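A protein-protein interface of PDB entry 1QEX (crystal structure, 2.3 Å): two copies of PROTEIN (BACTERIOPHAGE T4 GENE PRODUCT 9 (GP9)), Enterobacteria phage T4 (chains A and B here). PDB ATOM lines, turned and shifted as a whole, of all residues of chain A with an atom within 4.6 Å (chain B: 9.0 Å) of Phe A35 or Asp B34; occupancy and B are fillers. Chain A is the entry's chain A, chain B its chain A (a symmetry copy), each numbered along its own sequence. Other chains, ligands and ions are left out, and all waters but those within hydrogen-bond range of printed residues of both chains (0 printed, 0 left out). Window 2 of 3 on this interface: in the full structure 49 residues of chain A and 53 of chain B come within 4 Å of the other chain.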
ATOM      1  N   ILE A  31     -20.539  -7.761  14.582  1.00  0.00           N
ATOM      2  CA  ILE A  31     -20.888  -9.054  14.023  1.00  0.00           C
ATOM      3  C   ILE A  31     -22.226  -8.994  13.299  1.00  0.00           C
ATOM      4  O   ILE A  31     -22.444  -9.725  12.332  1.00  0.00           O
ATOM      5  CB  ILE A  31     -20.936 -10.145  15.120  1.00  0.00           C
ATOM      6  CG1 ILE A  31     -19.508 -10.486  15.558  1.00  0.00           C
ATOM      7  CG2 ILE A  31     -21.645 -11.393  14.604  1.00  0.00           C
ATOM      8  CD1 ILE A  31     -19.426 -11.537  16.647  1.00  0.00           C
ATOM      9  N   ASN A  32     -23.121  -8.122  13.756  1.00  0.00           N
ATOM     10  CA  ASN A  32     -24.426  -7.995  13.116  1.00  0.00           C
ATOM     11  C   ASN A  32     -24.338  -7.139  11.854  1.00  0.00           C
ATOM     12  O   ASN A  32     -25.186  -7.234  10.965  1.00  0.00           O
ATOM     13  CB  ASN A  32     -25.446  -7.391  14.086  1.00  0.00           C
ATOM     14  CG  ASN A  32     -25.753  -8.308  15.256  1.00  0.00           C
ATOM     15  OD1 ASN A  32     -24.862  -8.672  16.024  1.00  0.00           O
ATOM     16  ND2 ASN A  32     -27.018  -8.687  15.397  1.00  0.00           N
ATOM     17  N   SER A  33     -23.306  -6.304  11.779  1.00  0.00           N
ATOM     18  CA  SER A  33     -23.115  -5.440  10.623  1.00  0.00           C
ATOM     19  C   SER A  33     -22.571  -6.261   9.454  1.00  0.00           C
ATOM     20  O   SER A  33     -23.073  -6.174   8.334  1.00  0.00           O
ATOM     21  CB  SER A  33     -22.143  -4.312  10.968  1.00  0.00           C
ATOM     22  OG  SER A  33     -22.087  -3.355   9.926  1.00  0.00           O
ATOM     23  N   ASP A  34     -21.545  -7.061   9.729  1.00  0.00           N
ATOM     24  CA  ASP A  34     -20.935  -7.902   8.710  1.00  0.00           C
ATOM     25  C   ASP A  34     -21.917  -8.921   8.153  1.00  0.00           C
ATOM     26  O   ASP A  34     -22.143  -8.973   6.944  1.00  0.00           O
ATOM     27  CB  ASP A  34     -19.720  -8.633   9.274  1.00  0.00           C
ATOM     28  CG  ASP A  34     -18.576  -7.701   9.578  1.00  0.00           C
ATOM     29  OD1 ASP A  34     -18.684  -6.500   9.241  1.00  0.00           O
ATOM     30  OD2 ASP A  34     -17.565  -8.172  10.146  1.00  0.00           O
ATOM     31  N   PHE A  35     -22.491  -9.742   9.027  1.00  0.00           N
ATOM     32  CA  PHE A  35     -23.440 -10.746   8.573  1.00  0.00           C
ATOM     33  C   PHE A  35     -24.533 -10.111   7.726  1.00  0.00           C
ATOM     34  O   PHE A  35     -24.875 -10.625   6.663  1.00  0.00           O
ATOM     35  CB  PHE A  35     -24.065 -11.486   9.756  1.00  0.00           C
ATOM     36  CG  PHE A  35     -23.186 -12.562  10.322  1.00  0.00           C
ATOM     37  CD1 PHE A  35     -22.486 -13.419   9.477  1.00  0.00           C
ATOM     38  CD2 PHE A  35     -23.079 -12.741  11.697  1.00  0.00           C
ATOM     39  CE1 PHE A  35     -21.692 -14.439   9.992  1.00  0.00           C
ATOM     40  CE2 PHE A  35     -22.289 -13.760  12.223  1.00  0.00           C
ATOM     41  CZ  PHE A  35     -21.595 -14.610  11.369  1.00  0.00           C
ATOM     42  N   ASN A  36     -25.074  -8.992   8.193  1.00  0.00           N
ATOM     43  CA  ASN A  36     -26.118  -8.303   7.446  1.00  0.00           C
ATOM     44  C   ASN A  36     -25.638  -7.973   6.039  1.00  0.00           C
ATOM     45  O   ASN A  36     -26.402  -8.037   5.075  1.00  0.00           O
ATOM     46  CB  ASN A  36     -26.521  -7.022   8.169  1.00  0.00           C
ATOM     47  CG  ASN A  36     -27.595  -7.260   9.199  1.00  0.00           C
ATOM     48  OD1 ASN A  36     -27.513  -8.192   9.994  1.00  0.00           O
ATOM     49  ND2 ASN A  36     -28.616  -6.411   9.193  1.00  0.00           N
ATOM     50  N   ALA A  37     -24.360  -7.625   5.936  1.00  0.00           N
ATOM     51  CA  ALA A  37     -23.761  -7.289   4.657  1.00  0.00           C
ATOM     52  C   ALA A  37     -23.700  -8.532   3.774  1.00  0.00           C
ATOM     53  O   ALA A  37     -23.909  -8.455   2.567  1.00  0.00           O
ATOM     54  CB  ALA A  37     -22.363  -6.722   4.868  1.00  0.00           C
ATOM     55  N   ILE A  38     -23.424  -9.679   4.387  1.00  0.00           N
ATOM     56  CA  ILE A  38     -23.334 -10.937   3.655  1.00  0.00           C
ATOM     57  C   ILE A  38     -24.708 -11.484   3.267  1.00  0.00           C
ATOM     58  O   ILE A  38     -24.917 -11.885   2.125  1.00  0.00           O
ATOM     59  CB  ILE A  38     -22.579 -12.006   4.479  1.00  0.00           C
ATOM     60  CG1 ILE A  38     -21.146 -11.540   4.734  1.00  0.00           C
ATOM     61  CG2 ILE A  38     -22.574 -13.338   3.743  1.00  0.00           C
ATOM     62  CD1 ILE A  38     -20.330 -12.493   5.577  1.00  0.00           C
ATOM     63  N   TYR A  39     -25.644 -11.502   4.210  1.00  0.00           N
ATOM     64  CA  TYR A  39     -26.975 -12.012   3.915  1.00  0.00           C
ATOM     65  C   TYR A  39     -27.737 -11.153   2.913  1.00  0.00           C
ATOM     66  O   TYR A  39     -28.562 -11.670   2.163  1.00  0.00           O
ATOM     67  CB  TYR A  39     -27.805 -12.166   5.199  1.00  0.00           C
ATOM     68  CG  TYR A  39     -27.560 -13.464   5.943  1.00  0.00           C
ATOM     69  CD1 TYR A  39     -26.409 -13.648   6.703  1.00  0.00           C
ATOM     70  CD2 TYR A  39     -28.471 -14.516   5.864  1.00  0.00           C
ATOM     71  CE1 TYR A  39     -26.166 -14.850   7.368  1.00  0.00           C
ATOM     72  CE2 TYR A  39     -28.241 -15.721   6.522  1.00  0.00           C
ATOM     73  CZ  TYR A  39     -27.087 -15.880   7.273  1.00  0.00           C
ATOM     74  OH  TYR A  39     -26.849 -17.067   7.933  1.00  0.00           O
ATOM     75  N   GLY B  27     -25.161 -16.315  21.968  1.00  0.00           N
ATOM     76  CA  GLY B  27     -24.508 -15.547  20.926  1.00  0.00           C
ATOM     77  C   GLY B  27     -23.645 -16.467  20.081  1.00  0.00           C
ATOM     78  O   GLY B  27     -23.721 -16.454  18.850  1.00  0.00           O
ATOM     79  N   GLY B  28     -22.824 -17.271  20.751  1.00  0.00           N
ATOM     80  CA  GLY B  28     -21.959 -18.201  20.051  1.00  0.00           C
ATOM     81  C   GLY B  28     -22.746 -19.066  19.087  1.00  0.00           C
ATOM     82  O   GLY B  28     -22.517 -19.031  17.878  1.00  0.00           O
ATOM     83  N   ASN B  29     -23.683 -19.847  19.614  1.00  0.00           N
ATOM     84  CA  ASN B  29     -24.495 -20.707  18.763  1.00  0.00           C
ATOM     85  C   ASN B  29     -25.046 -19.922  17.574  1.00  0.00           C
ATOM     86  O   ASN B  29     -25.179 -20.465  16.475  1.00  0.00           O
ATOM     87  CB  ASN B  29     -25.648 -21.316  19.563  1.00  0.00           C
ATOM     88  CG  ASN B  29     -25.184 -22.394  20.523  1.00  0.00           C
ATOM     89  OD1 ASN B  29     -24.408 -22.130  21.442  1.00  0.00           O
ATOM     90  ND2 ASN B  29     -25.660 -23.618  20.312  1.00  0.00           N
ATOM     91  N   LYS B  30     -25.365 -18.648  17.792  1.00  0.00           N
ATOM     92  CA  LYS B  30     -25.887 -17.814  16.714  1.00  0.00           C
ATOM     93  C   LYS B  30     -24.809 -17.557  15.663  1.00  0.00           C
ATOM     94  O   LYS B  30     -25.079 -17.585  14.460  1.00  0.00           O
ATOM     95  CB  LYS B  30     -26.397 -16.474  17.255  1.00  0.00           C
ATOM     96  CG  LYS B  30     -27.755 -16.554  17.927  1.00  0.00           C
ATOM     97  CD  LYS B  30     -28.332 -15.162  18.170  1.00  0.00           C
ATOM     98  CE  LYS B  30     -29.687 -15.232  18.860  1.00  0.00           C
ATOM     99  NZ  LYS B  30     -30.336 -13.894  18.956  1.00  0.00           N
ATOM    100  N   ILE B  31     -23.590 -17.309  16.123  1.00  0.00           N
ATOM    101  CA  ILE B  31     -22.485 -17.055  15.217  1.00  0.00           C
ATOM    102  C   ILE B  31     -22.075 -18.326  14.486  1.00  0.00           C
ATOM    103  O   ILE B  31     -21.608 -18.265  13.347  1.00  0.00           O
ATOM    104  CB  ILE B  31     -21.266 -16.466  15.968  1.00  0.00           C
ATOM    105  CG1 ILE B  31     -21.561 -15.012  16.350  1.00  0.00           C
ATOM    106  CG2 ILE B  31     -20.014 -16.544  15.102  1.00  0.00           C
ATOM    107  CD1 ILE B  31     -20.440 -14.331  17.111  1.00  0.00           C
ATOM    108  N   ASN B  32     -22.251 -19.476  15.130  1.00  0.00           N
ATOM    109  CA  ASN B  32     -21.890 -20.742  14.499  1.00  0.00           C
ATOM    110  C   ASN B  32     -22.975 -21.199  13.527  1.00  0.00           C
ATOM    111  O   ASN B  32     -22.714 -21.985  12.613  1.00  0.00           O
ATOM    112  CB  ASN B  32     -21.649 -21.822  15.557  1.00  0.00           C
ATOM    113  CG  ASN B  32     -20.431 -21.536  16.417  1.00  0.00           C
ATOM    114  OD1 ASN B  32     -20.359 -20.506  17.089  1.00  0.00           O
ATOM    115  ND2 ASN B  32     -19.464 -22.447  16.399  1.00  0.00           N
ATOM    116  N   SER B  33     -24.192 -20.702  13.725  1.00  0.00           N
ATOM    117  CA  SER B  33     -25.306 -21.063  12.859  1.00  0.00           C
ATOM    118  C   SER B  33     -25.187 -20.315  11.532  1.00  0.00           C
ATOM    119  O   SER B  33     -25.306 -20.908  10.460  1.00  0.00           O
ATOM    120  CB  SER B  33     -26.629 -20.715  13.539  1.00  0.00           C
ATOM    121  OG  SER B  33     -27.726 -21.227  12.804  1.00  0.00           O
ATOM    122  N   ASP B  34     -24.944 -19.010  11.615  1.00  0.00           N
ATOM    123  CA  ASP B  34     -24.801 -18.180  10.429  1.00  0.00           C
ATOM    124  C   ASP B  34     -23.619 -18.609   9.575  1.00  0.00           C
ATOM    125  O   ASP B  34     -23.779 -18.905   8.390  1.00  0.00           O
ATOM    126  CB  ASP B  34     -24.634 -16.714  10.817  1.00  0.00           C
ATOM    127  CG  ASP B  34     -25.888 -16.127  11.410  1.00  0.00           C
ATOM    128  OD1 ASP B  34     -26.927 -16.827  11.413  1.00  0.00           O
ATOM    129  OD2 ASP B  34     -25.838 -14.962  11.865  1.00  0.00           O
ATOM    130  N   PHE B  35     -22.428 -18.632  10.166  1.00  0.00           N
ATOM    131  CA  PHE B  35     -21.247 -19.031   9.417  1.00  0.00           C
ATOM    132  C   PHE B  35     -21.467 -20.372   8.735  1.00  0.00           C
ATOM    133  O   PHE B  35     -21.147 -20.535   7.559  1.00  0.00           O
ATOM    134  CB  PHE B  35     -20.019 -19.104  10.324  1.00  0.00           C
ATOM    135  CG  PHE B  35     -19.399 -17.768  10.606  1.00  0.00           C
ATOM    136  CD1 PHE B  35     -19.243 -16.833   9.586  1.00  0.00           C
ATOM    137  CD2 PHE B  35     -18.946 -17.449  11.881  1.00  0.00           C
ATOM    138  CE1 PHE B  35     -18.641 -15.603   9.831  1.00  0.00           C
ATOM    139  CE2 PHE B  35     -18.342 -16.222  12.137  1.00  0.00           C
ATOM    140  CZ  PHE B  35     -18.189 -15.297  11.109  1.00  0.00           C
ATOM    141  N   ASN B  36     -22.019 -21.331   9.470  1.00  0.00           N
ATOM    142  CA  ASN B  36     -22.282 -22.647   8.903  1.00  0.00           C
ATOM    143  C   ASN B  36     -23.155 -22.525   7.661  1.00  0.00           C
ATOM    144  O   ASN B  36     -22.981 -23.259   6.687  1.00  0.00           O
ATOM    145  CB  ASN B  36     -22.969 -23.535   9.933  1.00  0.00           C
ATOM    146  CG  ASN B  36     -21.982 -24.256  10.815  1.00  0.00           C
ATOM    147  OD1 ASN B  36     -21.038 -23.660  11.326  1.00  0.00           O
ATOM    148  ND2 ASN B  36     -22.198 -25.552  11.004  1.00  0.00           N
ATOM    149  N   ALA B  37     -24.092 -21.585   7.707  1.00  0.00           N
ATOM    150  CA  ALA B  37     -24.994 -21.350   6.594  1.00  0.00           C
ATOM    151  C   ALA B  37     -24.213 -20.795   5.406  1.00  0.00           C
ATOM    152  O   ALA B  37     -24.491 -21.136   4.261  1.00  0.00           O
ATOM    153  CB  ALA B  37     -26.090 -20.377   7.008  1.00  0.00           C
ATOM    154  N   ILE B  38     -23.230 -19.946   5.690  1.00  0.00           N
ATOM    155  CA  ILE B  38     -22.414 -19.342   4.643  1.00  0.00           C
ATOM    156  C   ILE B  38     -21.391 -20.322   4.067  1.00  0.00           C
ATOM    157  O   ILE B  38     -21.250 -20.429   2.852  1.00  0.00           O
ATOM    158  CB  ILE B  38     -21.672 -18.091   5.171  1.00  0.00           C
ATOM    159  CG1 ILE B  38     -22.691 -17.035   5.600  1.00  0.00           C
ATOM    160  CG2 ILE B  38     -20.754 -17.528   4.097  1.00  0.00           C
ATOM    161  CD1 ILE B  38     -22.072 -15.784   6.179  1.00  0.00           C
ATOM    162  N   TYR B  39     -20.677 -21.036   4.932  1.00  0.00           N
ATOM    163  CA  TYR B  39     -19.683 -21.986   4.456  1.00  0.00           C
ATOM    164  C   TYR B  39     -20.290 -23.162   3.700  1.00  0.00           C
ATOM    165  O   TYR B  39     -19.653 -23.714   2.805  1.00  0.00           O
ATOM    166  CB  TYR B  39     -18.820 -22.509   5.615  1.00  0.00           C
ATOM    167  CG  TYR B  39     -17.661 -21.603   5.981  1.00  0.00           C
ATOM    168  CD1 TYR B  39     -17.868 -20.431   6.705  1.00  0.00           C
ATOM    169  CD2 TYR B  39     -16.360 -21.906   5.580  1.00  0.00           C
ATOM    170  CE1 TYR B  39     -16.810 -19.581   7.023  1.00  0.00           C
ATOM    171  CE2 TYR B  39     -15.296 -21.065   5.889  1.00  0.00           C
ATOM    172  CZ  TYR B  39     -15.527 -19.905   6.612  1.00  0.00           C
ATOM    173  OH  TYR B  39     -14.480 -19.066   6.929  1.00  0.00           O
ATOM    174  N   ASN B  40     -21.514 -23.550   4.045  1.00  0.00           N
ATOM    175  CA  ASN B  40     -22.139 -24.676   3.351  1.00  0.00           C
ATOM    176  C   ASN B  40     -22.784 -24.264   2.031  1.00  0.00           C
ATOM    177  O   ASN B  40     -23.159 -25.113   1.213  1.00  0.00           O
ATOM    178  CB  ASN B  40     -23.167 -25.366   4.246  1.00  0.00           C
ATOM    179  CG  ASN B  40     -22.522 -26.268   5.277  1.00  0.00           C
ATOM    180  OD1 ASN B  40     -21.971 -25.802   6.275  1.00  0.00           O
ATOM    181  ND2 ASN B  40     -22.580 -27.572   5.036  1.00  0.00           N
ATOM    182  N   ALA B  41     -22.913 -22.959   1.829  1.00  0.00           N
ATOM    183  CA  ALA B  41     -23.482 -22.444   0.596  1.00  0.00           C
ATOM    184  C   ALA B  41     -22.344 -22.243  -0.401  1.00  0.00           C
ATOM    185  O   ALA B  41     -22.554 -22.294  -1.613  1.00  0.00           O
ATOM    186  CB  ALA B  41     -24.195 -21.126   0.854  1.00  0.00           C
ATOM    187  N   PHE B  42     -21.137 -22.026   0.121  1.00  0.00           N
ATOM    188  CA  PHE B  42     -19.964 -21.807  -0.717  1.00  0.00           C
ATOM    189  C   PHE B  42     -18.844 -22.810  -0.458  1.00  0.00           C
ATOM    190  O   PHE B  42     -17.692 -22.562  -0.814  1.00  0.00           O
ATOM    191  CB  PHE B  42     -19.428 -20.389  -0.504  1.00  0.00           C
ATOM    192  CG  PHE B  42     -20.437 -19.311  -0.766  1.00  0.00           C
ATOM    193  CD1 PHE B  42     -21.057 -19.205  -2.007  1.00  0.00           C
ATOM    194  CD2 PHE B  42     -20.747 -18.378   0.220  1.00  0.00           C
ATOM    195  CE1 PHE B  42     -21.973 -18.180  -2.265  1.00  0.00           C
ATOM    196  CE2 PHE B  42     -21.660 -17.350  -0.024  1.00  0.00           C
ATOM    197  CZ  PHE B  42     -22.273 -17.251  -1.269  1.00  0.00           C
ATOM    198  N   GLN B  59     -13.882 -26.865   5.874  1.00  0.00           N
ATOM    199  CA  GLN B  59     -14.584 -26.125   4.834  1.00  0.00           C
ATOM    200  C   GLN B  59     -13.963 -24.759   4.572  1.00  0.00           C
ATOM    201  O   GLN B  59     -13.454 -24.113   5.486  1.00  0.00           O
ATOM    202  CB  GLN B  59     -16.049 -25.941   5.222  1.00  0.00           C
ATOM    203  CG  GLN B  59     -16.891 -27.196   5.095  1.00  0.00           C
ATOM    204  CD  GLN B  59     -18.321 -26.986   5.553  1.00  0.00           C
ATOM    205  OE1 GLN B  59     -19.195 -27.816   5.297  1.00  0.00           O
ATOM    206  NE2 GLN B  59     -18.566 -25.874   6.242  1.00  0.00           N
ATOM    207  N   ILE B  61     -14.351 -21.017   1.892  1.00  0.00           N
ATOM    208  CA  ILE B  61     -15.253 -20.245   1.038  1.00  0.00           C
ATOM    209  C   ILE B  61     -14.712 -20.187  -0.391  1.00  0.00           C
ATOM    210  O   ILE B  61     -13.678 -19.567  -0.643  1.00  0.00           O
ATOM    211  CB  ILE B  61     -15.409 -18.789   1.537  1.00  0.00           C
ATOM    212  CG1 ILE B  61     -15.872 -18.767   2.997  1.00  0.00           C
ATOM    213  CG2 ILE B  61     -16.390 -18.042   0.642  1.00  0.00           C
ATOM    214  CD1 ILE B  61     -17.232 -19.389   3.238  1.00  0.00           C
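Ile B31 touches its own counterpart, Ile A31. Phe A35 touches Asp B34, but with the chains exchanged Asp A34 does not touch Phe B35 (7.1 Å). Tyr A39 touches Asp B34, but with the chains exchanged Asp A34 does not touch Tyr B39 (11.5 Å). Tyr A39 touches Ala B37, but with the chains exchanged Ala A37 does not touch Tyr B39 (12.9 Å). Of the 6 pairs that touch across the chains among the printed residues, 3 have their exchanged pair printed and touching as well.
Phe A35 touches two residues of chain B. Of chain A, only Phe A35 (3.5 Å) and Tyr A39 (3.4 Å) come within 4 Å of Asp B34. Of chain B, only Ile B38 comes within 4 Å of Ile A38. Of the printed residues of chain A, Ile B38 touches Ile A38 (3.5 Å). Of the printed residues of chain B, Tyr A39 touches Asp B34 (3.4 Å) and Ala B37 (3.5 Å). Printed residues of chain B within 4 Å of Ile A31: Ile B31 (3.0 Å). Of the printed residues of chain A, Ile B31 touches Ile A31 (3.0 Å). Of the printed residues of chain A, Phe B35 touches Phe A35.
Among the printed residues, merely in contact across the chains: Ile A31 with Ile B31 (3.0 Å), Phe A35 with Phe B35 (3.3 Å), Ile A38 with Ile B38 (3.5 Å), Tyr A39 with Ala B37 (3.5 Å) and Phe A35 with Asp B34 (3.5 Å).
Of the 18 printed residues of chain B, 5 touch a printed residue of chain A. Hydrophobic or aromatic side chains of chain B that line the printed part of chain A: Ile B31, Phe B35, Ala B37 and Ile B38. Hydrophobic or aromatic side chains of chain A within 4 Å of the printed part of chain B: Ile A31, Phe A35, Ile A38 and Tyr A39. Among the printed residues, no Asp or Glu carboxylate lies within 4 Å of a Lys or Arg side-chain nitrogen of the other chain.
OH of Tyr A39 sits close to OD1 of Asp B34, at 3.5 Å.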
